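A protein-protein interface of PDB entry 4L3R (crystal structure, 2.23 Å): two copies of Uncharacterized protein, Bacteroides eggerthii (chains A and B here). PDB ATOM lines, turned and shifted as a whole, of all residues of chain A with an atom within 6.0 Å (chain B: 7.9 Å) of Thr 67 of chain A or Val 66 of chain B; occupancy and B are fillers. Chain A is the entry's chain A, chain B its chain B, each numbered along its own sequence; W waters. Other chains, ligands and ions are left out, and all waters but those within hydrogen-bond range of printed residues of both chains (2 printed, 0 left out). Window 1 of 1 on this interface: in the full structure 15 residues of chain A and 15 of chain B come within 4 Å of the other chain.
The backbone NH (N) of Ile 86 of chain A sits at hydrogen-bond distance from the backbone carbonyl oxygen (O) of Gly 64 of chain B (3.2 Å).
SD of Met 7 of chain A sits close to O of Cys 59 of chain B.
N of Gly 68 of chain A lies within hydrogen-bond range of O of Val 66 of chain B (2.9 Å).
O of Ile 86 of chain B sits close to OD1 of Asp 61 of chain A.
The backbone carbonyl oxygen (O) of Val 66 of chain A is in hydrogen-bond range of the backbone NH (N) of Gly 68 of chain B (2.8 Å).
The backbone carbonyl oxygen (O) of Ile 86 of chain A lies close to the side-chain carboxylate (OD1) of Asp 61 of chain B (2.9 Å).
The side-chain sulfur (SD) of Met 7 of chain B lies close to the backbone carbonyl oxygen (O) of Cys 59 of chain A (3.8 Å).
The side-chain sulfur of Cys 59 of chain A is disulfide-bonded to the side-chain sulfur of Cys 59 of chain B.
The backbone NH (N) of Thr 67 of chain A lies within hydrogen-bond range of the backbone carbonyl oxygen (O) of Ala 60 of chain A (2.9 Å).
The side-chain carboxylate (OD1) of Asp 61 of chain B lies within hydrogen-bond range of the backbone NH (N) of Glu 65 of chain B, at 3.1 Å.
The backbone NH (N) of Thr 67 of chain B lies within hydrogen-bond range of the backbone carbonyl oxygen (O) of Ala 60 of chain B (2.9 Å).
The side-chain carboxylate of Asp 61 of chain A sits at hydrogen-bond distance from the backbone NH of Glu 65 of chain A.
Among the printed residues, merely in contact across the chains: Asp 61 of chain A with Met 7 of chain B (3.3 Å), Met 7 of chain A with Asp 61 of chain B (3.3 Å), Val 66 of chain A with Thr 67 of chain B (3.6 Å), Thr 67 of chain A with Val 66 of chain B (3.6 Å), Ile 86 of chain A with Glu 65 of chain B (3.6 Å), Val 66 of chain A with Ile 86 of chain B (3.7 Å), Ile 86 of chain A with Val 66 of chain B (3.7 Å), Glu 65 of chain A with Ile 86 of chain B (3.7 Å), Val 66 of chain A with Phe 10 of chain B (3.8 Å), Met 7 of chain A with Ala 60 of chain B (3.8 Å), Val 6 of chain A with Asp 61 of chain B (3.8 Å), Phe 10 of chain A with Val 66 of chain B (3.8 Å), Ala 60 of chain A with Met 7 of chain B (3.8 Å), Val 66 of chain A with Met 7 of chain B (3.9 Å) and Met 7 of chain A with Val 66 of chain B (3.9 Å).
Printed residues of chain A within 4 Å of Val 66 of chain B: Met 7, Phe 10, Thr 67, Gly 68 and Ile 86.
Of the printed residues of chain B, Gly 68 of chain A touches Val 66.
Of the printed residues of chain B, Asp 61 of chain A touches Met 7 (3.3 Å) and Ile 86 (2.8 Å).
Of the printed residues of chain A, Glu 65 of chain B touches Ile 86.
The nearest residue of chain B that does not touch Thr 67 of chain A is Thr 67 of chain B (4.5 Å).
The nearest printed residue of chain A that does not touch Val 66 of chain B is Cys 59 of chain A (4.1 Å).
Hydrophobic or aromatic side chains of chain B within 4 Å of the printed part of chain A: Met 7, Phe 10, Val 66 and Ile 86.
Of the 15 printed residues of chain A, 11 touch a printed residue of chain B.
Among the printed residues, 23 pairs touch across the chains.
Met 7 of chain A touches Val 66 of chain B, and with the chains exchanged Val 66 of chain A touches Met 7 of chain B.
Cys 59 of chain B touches its own counterpart, Cys 59 of chain A.
Glu 65 of chain A touches Ile 86 of chain B, and with the chains exchanged Ile 86 of chain A touches Glu 65 of chain B.
Val 66 of chain A touches Gly 68 of chain B, and with the chains exchanged Gly 68 of chain A touches Val 66 of chain B.
Positions printed for both chains: 7, 10, 58, 59, 60, 61, 62, 65, 66, 67, 68, 69 and 86.
Of the 23 pairs that touch across the chains among the printed residues, 21 have their exchanged pair printed and touching as well.
Water W2 lies within hydrogen-bond range of O of Leu 84 of chain A (2.8 Å), O of Gly 68 of chain A (2.9 Å) and N of Val 66 of chain B (2.9 Å).
Water W1 lies within hydrogen-bond range of the backbone NH of Val 66 of chain A (2.8 Å) and the backbone carbonyl oxygen of Gly 68 of chain B (2.9 Å).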
ATOM      1  N   VAL A   6      17.911  -0.220   5.941  1.00  0.00           N
ATOM      2  CA  VAL A   6      17.434  -1.376   6.712  1.00  0.00           C
ATOM      3  C   VAL A   6      18.533  -1.944   7.605  1.00  0.00           C
ATOM      4  O   VAL A   6      18.272  -2.184   8.778  1.00  0.00           O
ATOM      5  CB  VAL A   6      16.857  -2.489   5.787  1.00  0.00           C
ATOM      6  CG1 VAL A   6      16.615  -3.799   6.547  1.00  0.00           C
ATOM      7  CG2 VAL A   6      15.565  -2.026   5.136  1.00  0.00           C
ATOM      8  N   MET A   7      19.747  -2.147   7.062  1.00  0.00           N
ATOM      9  CA  MET A   7      20.812  -2.765   7.854  1.00  0.00           C
ATOM     10  C   MET A   7      21.314  -1.850   8.986  1.00  0.00           C
ATOM     11  O   MET A   7      21.933  -2.369   9.915  1.00  0.00           O
ATOM     12  CB  MET A   7      21.973  -3.272   6.967  1.00  0.00           C
ATOM     13  CG  MET A   7      22.052  -4.814   6.909  1.00  0.00           C
ATOM     14  SD  MET A   7      20.322  -5.769   6.683  1.00  0.00           S
ATOM     15  CE  MET A   7      19.823  -4.984   5.079  1.00  0.00           C
ATOM     16  N   PHE A  10      19.912  -3.022  12.346  1.00  0.00           N
ATOM     17  CA  PHE A  10      20.657  -4.171  12.879  1.00  0.00           C
ATOM     18  C   PHE A  10      22.076  -3.799  13.386  1.00  0.00           C
ATOM     19  O   PHE A  10      22.722  -4.637  14.015  1.00  0.00           O
ATOM     20  CB  PHE A  10      20.835  -5.239  11.760  1.00  0.00           C
ATOM     21  CG  PHE A  10      19.580  -5.943  11.286  1.00  0.00           C
ATOM     22  CD1 PHE A  10      18.649  -5.283  10.490  1.00  0.00           C
ATOM     23  CD2 PHE A  10      19.390  -7.299  11.529  1.00  0.00           C
ATOM     24  CE1 PHE A  10      17.521  -5.947  10.009  1.00  0.00           C
ATOM     25  CE2 PHE A  10      18.262  -7.960  11.048  1.00  0.00           C
ATOM     26  CZ  PHE A  10      17.324  -7.276  10.315  1.00  0.00           C
ATOM     27  N   ASN A  58      18.557  -8.922  14.778  1.00  0.00           N
ATOM     28  CA  ASN A  58      19.828  -9.658  14.692  1.00  0.00           C
ATOM     29  C   ASN A  58      19.855 -10.626  13.533  1.00  0.00           C
ATOM     30  O   ASN A  58      18.815 -11.014  13.022  1.00  0.00           O
ATOM     31  CB  ASN A  58      20.072 -10.469  15.975  1.00  0.00           C
ATOM     32  CG  ASN A  58      19.897  -9.721  17.273  1.00  0.00           C
ATOM     33  OD1 ASN A  58      19.023 -10.045  18.081  1.00  0.00           O
ATOM     34  ND2 ASN A  58      20.756  -8.746  17.526  1.00  0.00           N
ATOM     35  N   CYS A  59      21.050 -11.097  13.180  1.00  0.00           N
ATOM     36  CA  CYS A  59      21.219 -12.146  12.176  1.00  0.00           C
ATOM     37  C   CYS A  59      21.564 -13.420  12.922  1.00  0.00           C
ATOM     38  O   CYS A  59      22.293 -13.364  13.910  1.00  0.00           O
ATOM     39  CB  CYS A  59      22.264 -11.773  11.133  1.00  0.00           C
ATOM     40  SG  CYS A  59      21.614 -10.735   9.792  1.00  0.00           S
ATOM     41  N   ALA A  60      20.957 -14.545  12.525  1.00  0.00           N
ATOM     42  CA  ALA A  60      21.131 -15.818  13.219  1.00  0.00           C
ATOM     43  C   ALA A  60      21.166 -16.984  12.253  1.00  0.00           C
ATOM     44  O   ALA A  60      20.485 -16.931  11.234  1.00  0.00           O
ATOM     45  CB  ALA A  60      19.979 -16.010  14.199  1.00  0.00           C
ATOM     46  N   ASP A  61      21.894 -18.063  12.611  1.00  0.00           N
ATOM     47  CA  ASP A  61      21.985 -19.270  11.793  1.00  0.00           C
ATOM     48  C   ASP A  61      20.799 -20.163  12.142  1.00  0.00           C
ATOM     49  O   ASP A  61      20.834 -20.889  13.140  1.00  0.00           O
ATOM     50  CB  ASP A  61      23.328 -19.997  11.993  1.00  0.00           C
ATOM     51  CG  ASP A  61      23.484 -21.258  11.168  1.00  0.00           C
ATOM     52  OD1 ASP A  61      23.010 -21.274  10.018  1.00  0.00           O
ATOM     53  OD2 ASP A  61      24.105 -22.216  11.666  1.00  0.00           O
ATOM     54  N   VAL A  62      19.728 -20.052  11.342  1.00  0.00           N
ATOM     55  CA  VAL A  62      18.485 -20.795  11.515  1.00  0.00           C
ATOM     56  C   VAL A  62      18.426 -21.906  10.466  1.00  0.00           C
ATOM     57  O   VAL A  62      18.254 -21.619   9.283  1.00  0.00           O
ATOM     58  CB  VAL A  62      17.256 -19.844  11.408  1.00  0.00           C
ATOM     59  CG1 VAL A  62      15.949 -20.596  11.666  1.00  0.00           C
ATOM     60  CG2 VAL A  62      17.388 -18.653  12.358  1.00  0.00           C
ATOM     61  N   GLU A  65      21.285 -21.876   7.466  1.00  0.00           N
ATOM     62  CA  GLU A  65      21.394 -20.637   6.683  1.00  0.00           C
ATOM     63  C   GLU A  65      21.191 -19.435   7.607  1.00  0.00           C
ATOM     64  O   GLU A  65      20.445 -19.541   8.573  1.00  0.00           O
ATOM     65  CB  GLU A  65      20.393 -20.626   5.511  1.00  0.00           C
ATOM     66  CG  GLU A  65      18.930 -20.743   5.919  1.00  0.00           C
ATOM     67  CD  GLU A  65      17.951 -20.683   4.762  1.00  0.00           C
ATOM     68  OE1 GLU A  65      18.204 -21.343   3.727  1.00  0.00           O
ATOM     69  OE2 GLU A  65      16.920 -19.986   4.896  1.00  0.00           O
ATOM     70  N   VAL A  66      21.865 -18.309   7.330  1.00  0.00           N
ATOM     71  CA  VAL A  66      21.785 -17.118   8.176  1.00  0.00           C
ATOM     72  C   VAL A  66      20.625 -16.227   7.708  1.00  0.00           C
ATOM     73  O   VAL A  66      20.560 -15.859   6.535  1.00  0.00           O
ATOM     74  CB  VAL A  66      23.143 -16.371   8.206  1.00  0.00           C
ATOM     75  CG1 VAL A  66      23.037 -15.041   8.961  1.00  0.00           C
ATOM     76  CG2 VAL A  66      24.221 -17.257   8.823  1.00  0.00           C
ATOM     77  N   THR A  67      19.715 -15.888   8.639  1.00  0.00           N
ATOM     78  CA  THR A  67      18.538 -15.060   8.371  1.00  0.00           C
ATOM     79  C   THR A  67      18.441 -13.918   9.381  1.00  0.00           C
ATOM     80  O   THR A  67      18.856 -14.074  10.528  1.00  0.00           O
ATOM     81  CB  THR A  67      17.253 -15.927   8.439  1.00  0.00           C
ATOM     82  OG1 THR A  67      17.057 -16.385   9.776  1.00  0.00           O
ATOM     83  CG2 THR A  67      17.293 -17.128   7.499  1.00  0.00           C
ATOM     84  N   GLY A  68      17.858 -12.803   8.961  1.00  0.00           N
ATOM     85  CA  GLY A  68      17.606 -11.668   9.841  1.00  0.00           C
ATOM     86  C   GLY A  68      16.338 -11.955  10.621  1.00  0.00           C
ATOM     87  O   GLY A  68      15.344 -12.391  10.034  1.00  0.00           O
ATOM     88  N   THR A  69      16.383 -11.798  11.950  1.00  0.00           N
ATOM     89  CA  THR A  69      15.244 -12.088  12.827  1.00  0.00           C
ATOM     90  C   THR A  69      15.034 -10.967  13.828  1.00  0.00           C
ATOM     91  O   THR A  69      15.857 -10.055  13.919  1.00  0.00           O
ATOM     92  CB  THR A  69      15.481 -13.410  13.570  1.00  0.00           C
ATOM     93  OG1 THR A  69      16.557 -13.236  14.495  1.00  0.00           O
ATOM     94  CG2 THR A  69      15.757 -14.578  12.628  1.00  0.00           C
ATOM     95  N   LEU A  84      11.140 -12.543  10.446  1.00  0.00           N
ATOM     96  CA  LEU A  84      11.043 -11.152  10.024  1.00  0.00           C
ATOM     97  C   LEU A  84      10.957 -11.013   8.507  1.00  0.00           C
ATOM     98  O   LEU A  84      11.722 -11.635   7.773  1.00  0.00           O
ATOM     99  CB  LEU A  84      12.277 -10.383  10.535  1.00  0.00           C
ATOM    100  CG  LEU A  84      12.433  -8.919  10.078  1.00  0.00           C
ATOM    101  CD1 LEU A  84      11.354  -8.039  10.674  1.00  0.00           C
ATOM    102  CD2 LEU A  84      13.813  -8.402  10.400  1.00  0.00           C
ATOM    103  N   ILE A  86      10.965  -7.621   5.997  1.00  0.00           N
ATOM    104  CA  ILE A  86      11.181  -6.181   6.053  1.00  0.00           C
ATOM    105  C   ILE A  86      11.565  -5.715   4.662  1.00  0.00           C
ATOM    106  O   ILE A  86      12.278  -6.422   3.952  1.00  0.00           O
ATOM    107  CB  ILE A  86      12.218  -5.809   7.148  1.00  0.00           C
ATOM    108  CG1 ILE A  86      12.306  -4.284   7.331  1.00  0.00           C
ATOM    109  CG2 ILE A  86      13.591  -6.414   6.847  1.00  0.00           C
ATOM    110  CD1 ILE A  86      12.976  -3.864   8.588  1.00  0.00           C
ATOM    111  N   MET B   7      28.132 -16.224  13.911  1.00  0.00           N
ATOM    112  CA  MET B   7      27.888 -14.794  13.729  1.00  0.00           C
ATOM    113  C   MET B   7      29.142 -13.964  14.022  1.00  0.00           C
ATOM    114  O   MET B   7      29.168 -12.800  13.635  1.00  0.00           O
ATOM    115  CB  MET B   7      26.672 -14.308  14.533  1.00  0.00           C
ATOM    116  CG  MET B   7      25.450 -14.007  13.644  1.00  0.00           C
ATOM    117  SD  MET B   7      25.007 -15.369  12.272  1.00  0.00           S
ATOM    118  CE  MET B   7      24.824 -16.827  13.500  1.00  0.00           C
ATOM    119  N   PHE B  10      30.468 -12.854  10.625  1.00  0.00           N
ATOM    120  CA  PHE B  10      29.757 -11.690  10.063  1.00  0.00           C
ATOM    121  C   PHE B  10      29.999 -10.380  10.839  1.00  0.00           C
ATOM    122  O   PHE B  10      29.608  -9.312  10.356  1.00  0.00           O
ATOM    123  CB  PHE B  10      28.234 -11.944  10.099  1.00  0.00           C
ATOM    124  CG  PHE B  10      27.712 -12.942   9.102  1.00  0.00           C
ATOM    125  CD1 PHE B  10      27.845 -14.304   9.325  1.00  0.00           C
ATOM    126  CD2 PHE B  10      26.999 -12.524   7.983  1.00  0.00           C
ATOM    127  CE1 PHE B  10      27.354 -15.226   8.407  1.00  0.00           C
ATOM    128  CE2 PHE B  10      26.490 -13.452   7.077  1.00  0.00           C
ATOM    129  CZ  PHE B  10      26.677 -14.795   7.291  1.00  0.00           C
ATOM    130  N   ASN B  58      28.019 -10.950   4.836  1.00  0.00           N
ATOM    131  CA  ASN B  58      27.111  -9.843   5.153  1.00  0.00           C
ATOM    132  C   ASN B  58      25.668 -10.266   5.171  1.00  0.00           C
ATOM    133  O   ASN B  58      25.291 -11.249   4.532  1.00  0.00           O
ATOM    134  CB  ASN B  58      27.247  -8.708   4.129  1.00  0.00           C
ATOM    135  CG  ASN B  58      28.653  -8.259   3.839  1.00  0.00           C
ATOM    136  OD1 ASN B  58      29.137  -8.385   2.713  1.00  0.00           O
ATOM    137  ND2 ASN B  58      29.316  -7.676   4.830  1.00  0.00           N
ATOM    138  N   CYS B  59      24.855  -9.448   5.851  1.00  0.00           N
ATOM    139  CA  CYS B  59      23.415  -9.590   5.909  1.00  0.00           C
ATOM    140  C   CYS B  59      22.835  -8.500   5.020  1.00  0.00           C
ATOM    141  O   CYS B  59      23.277  -7.352   5.104  1.00  0.00           O
ATOM    142  CB  CYS B  59      22.905  -9.497   7.343  1.00  0.00           C
ATOM    143  SG  CYS B  59      22.892 -11.081   8.224  1.00  0.00           S
ATOM    144  N   ALA B  60      21.902  -8.861   4.135  1.00  0.00           N
ATOM    145  CA  ALA B  60      21.312  -7.921   3.186  1.00  0.00           C
ATOM    146  C   ALA B  60      19.834  -8.183   2.992  1.00  0.00           C
ATOM    147  O   ALA B  60      19.400  -9.326   3.106  1.00  0.00           O
ATOM    148  CB  ALA B  60      22.030  -8.041   1.848  1.00  0.00           C
ATOM    149  N   ASP B  61      19.082  -7.134   2.624  1.00  0.00           N
ATOM    150  CA  ASP B  61      17.642  -7.220   2.397  1.00  0.00           C
ATOM    151  C   ASP B  61      17.386  -7.684   0.948  1.00  0.00           C
ATOM    152  O   ASP B  61      17.306  -6.867   0.030  1.00  0.00           O
ATOM    153  CB  ASP B  61      16.962  -5.868   2.703  1.00  0.00           C
ATOM    154  CG  ASP B  61      15.453  -5.880   2.636  1.00  0.00           C
ATOM    155  OD1 ASP B  61      14.866  -6.978   2.676  1.00  0.00           O
ATOM    156  OD2 ASP B  61      14.858  -4.790   2.569  1.00  0.00           O
ATOM    157  N   VAL B  62      17.264  -9.014   0.769  1.00  0.00           N
ATOM    158  CA  VAL B  62      17.044  -9.679  -0.516  1.00  0.00           C
ATOM    159  C   VAL B  62      15.610 -10.193  -0.612  1.00  0.00           C
ATOM    160  O   VAL B  62      15.272 -11.128   0.106  1.00  0.00           O
ATOM    161  CB  VAL B  62      18.042 -10.868  -0.672  1.00  0.00           C
ATOM    162  CG1 VAL B  62      17.850 -11.580  -2.016  1.00  0.00           C
ATOM    163  CG2 VAL B  62      19.490 -10.411  -0.494  1.00  0.00           C
ATOM    164  N   ASN B  63      14.792  -9.643  -1.529  1.00  0.00           N
ATOM    165  CA  ASN B  63      13.421 -10.107  -1.783  1.00  0.00           C
ATOM    166  C   ASN B  63      12.510  -9.928  -0.542  1.00  0.00           C
ATOM    167  O   ASN B  63      11.789 -10.852  -0.155  1.00  0.00           O
ATOM    168  CB  ASN B  63      13.442 -11.597  -2.258  1.00  0.00           C
ATOM    169  CG  ASN B  63      12.287 -12.037  -3.147  1.00  0.00           C
ATOM    170  OD1 ASN B  63      11.603 -11.231  -3.796  1.00  0.00           O
ATOM    171  ND2 ASN B  63      12.086 -13.348  -3.250  1.00  0.00           N
ATOM    172  N   GLY B  64      12.536  -8.728   0.042  1.00  0.00           N
ATOM    173  CA  GLY B  64      11.720  -8.391   1.208  1.00  0.00           C
ATOM    174  C   GLY B  64      12.022  -9.167   2.481  1.00  0.00           C
ATOM    175  O   GLY B  64      11.150  -9.316   3.334  1.00  0.00           O
ATOM    176  N   GLU B  65      13.248  -9.671   2.629  1.00  0.00           N
ATOM    177  CA  GLU B  65      13.656 -10.404   3.826  1.00  0.00           C
ATOM    178  C   GLU B  65      15.170 -10.334   3.941  1.00  0.00           C
ATOM    179  O   GLU B  65      15.844 -10.268   2.922  1.00  0.00           O
ATOM    180  CB  GLU B  65      13.138 -11.859   3.802  1.00  0.00           C
ATOM    181  CG  GLU B  65      13.913 -12.810   2.904  1.00  0.00           C
ATOM    182  CD  GLU B  65      13.248 -14.145   2.628  1.00  0.00           C
ATOM    183  OE1 GLU B  65      12.001 -14.190   2.522  1.00  0.00           O
ATOM    184  OE2 GLU B  65      13.989 -15.141   2.460  1.00  0.00           O
ATOM    185  N   VAL B  66      15.699 -10.314   5.168  1.00  0.00           N
ATOM    186  CA  VAL B  66      17.135 -10.194   5.407  1.00  0.00           C
ATOM    187  C   VAL B  66      17.775 -11.588   5.419  1.00  0.00           C
ATOM    188  O   VAL B  66      17.333 -12.464   6.163  1.00  0.00           O
ATOM    189  CB  VAL B  66      17.415  -9.391   6.703  1.00  0.00           C
ATOM    190  CG1 VAL B  66      18.903  -9.392   7.062  1.00  0.00           C
ATOM    191  CG2 VAL B  66      16.898  -7.963   6.563  1.00  0.00           C
ATOM    192  N   THR B  67      18.810 -11.788   4.581  1.00  0.00           N
ATOM    193  CA  THR B  67      19.536 -13.061   4.491  1.00  0.00           C
ATOM    194  C   THR B  67      21.047 -12.836   4.553  1.00  0.00           C
ATOM    195  O   THR B  67      21.533 -11.799   4.115  1.00  0.00           O
ATOM    196  CB  THR B  67      19.186 -13.817   3.185  1.00  0.00           C
ATOM    197  OG1 THR B  67      19.774 -13.142   2.076  1.00  0.00           O
ATOM    198  CG2 THR B  67      17.680 -13.969   2.967  1.00  0.00           C
ATOM    199  N   GLY B  68      21.762 -13.831   5.070  1.00  0.00           N
ATOM    200  CA  GLY B  68      23.218 -13.829   5.122  1.00  0.00           C
ATOM    201  C   GLY B  68      23.768 -14.336   3.801  1.00  0.00           C
ATOM    202  O   GLY B  68      23.318 -15.376   3.308  1.00  0.00           O
ATOM    203  N   THR B  69      24.700 -13.584   3.194  1.00  0.00           N
ATOM    204  CA  THR B  69      25.312 -13.931   1.909  1.00  0.00           C
ATOM    205  C   THR B  69      26.817 -13.743   1.971  1.00  0.00           C
ATOM    206  O   THR B  69      27.337 -13.209   2.952  1.00  0.00           O
ATOM    207  CB  THR B  69      24.732 -13.068   0.769  1.00  0.00           C
ATOM    208  OG1 THR B  69      25.041 -11.701   1.015  1.00  0.00           O
ATOM    209  CG2 THR B  69      23.242 -13.251   0.585  1.00  0.00           C
ATOM    210  N   ILE B  86      25.450 -22.327   5.751  1.00  0.00           N
ATOM    211  CA  ILE B  86      26.496 -22.461   6.772  1.00  0.00           C
ATOM    212  C   ILE B  86      25.884 -23.059   8.022  1.00  0.00           C
ATOM    213  O   ILE B  86      24.797 -22.652   8.409  1.00  0.00           O
ATOM    214  CB  ILE B  86      27.207 -21.101   7.051  1.00  0.00           C
ATOM    215  CG1 ILE B  86      28.465 -21.311   7.919  1.00  0.00           C
ATOM    216  CG2 ILE B  86      26.261 -20.077   7.691  1.00  0.00           C
ATOM    217  CD1 ILE B  86      29.337 -20.123   7.986  1.00  0.00           C
HETATM  218  O   HOH W   1      22.796 -17.828   4.694  1.00  0.00           O
HETATM  219  O   HOH W   2      14.465 -11.430   7.494  1.00  0.00           O
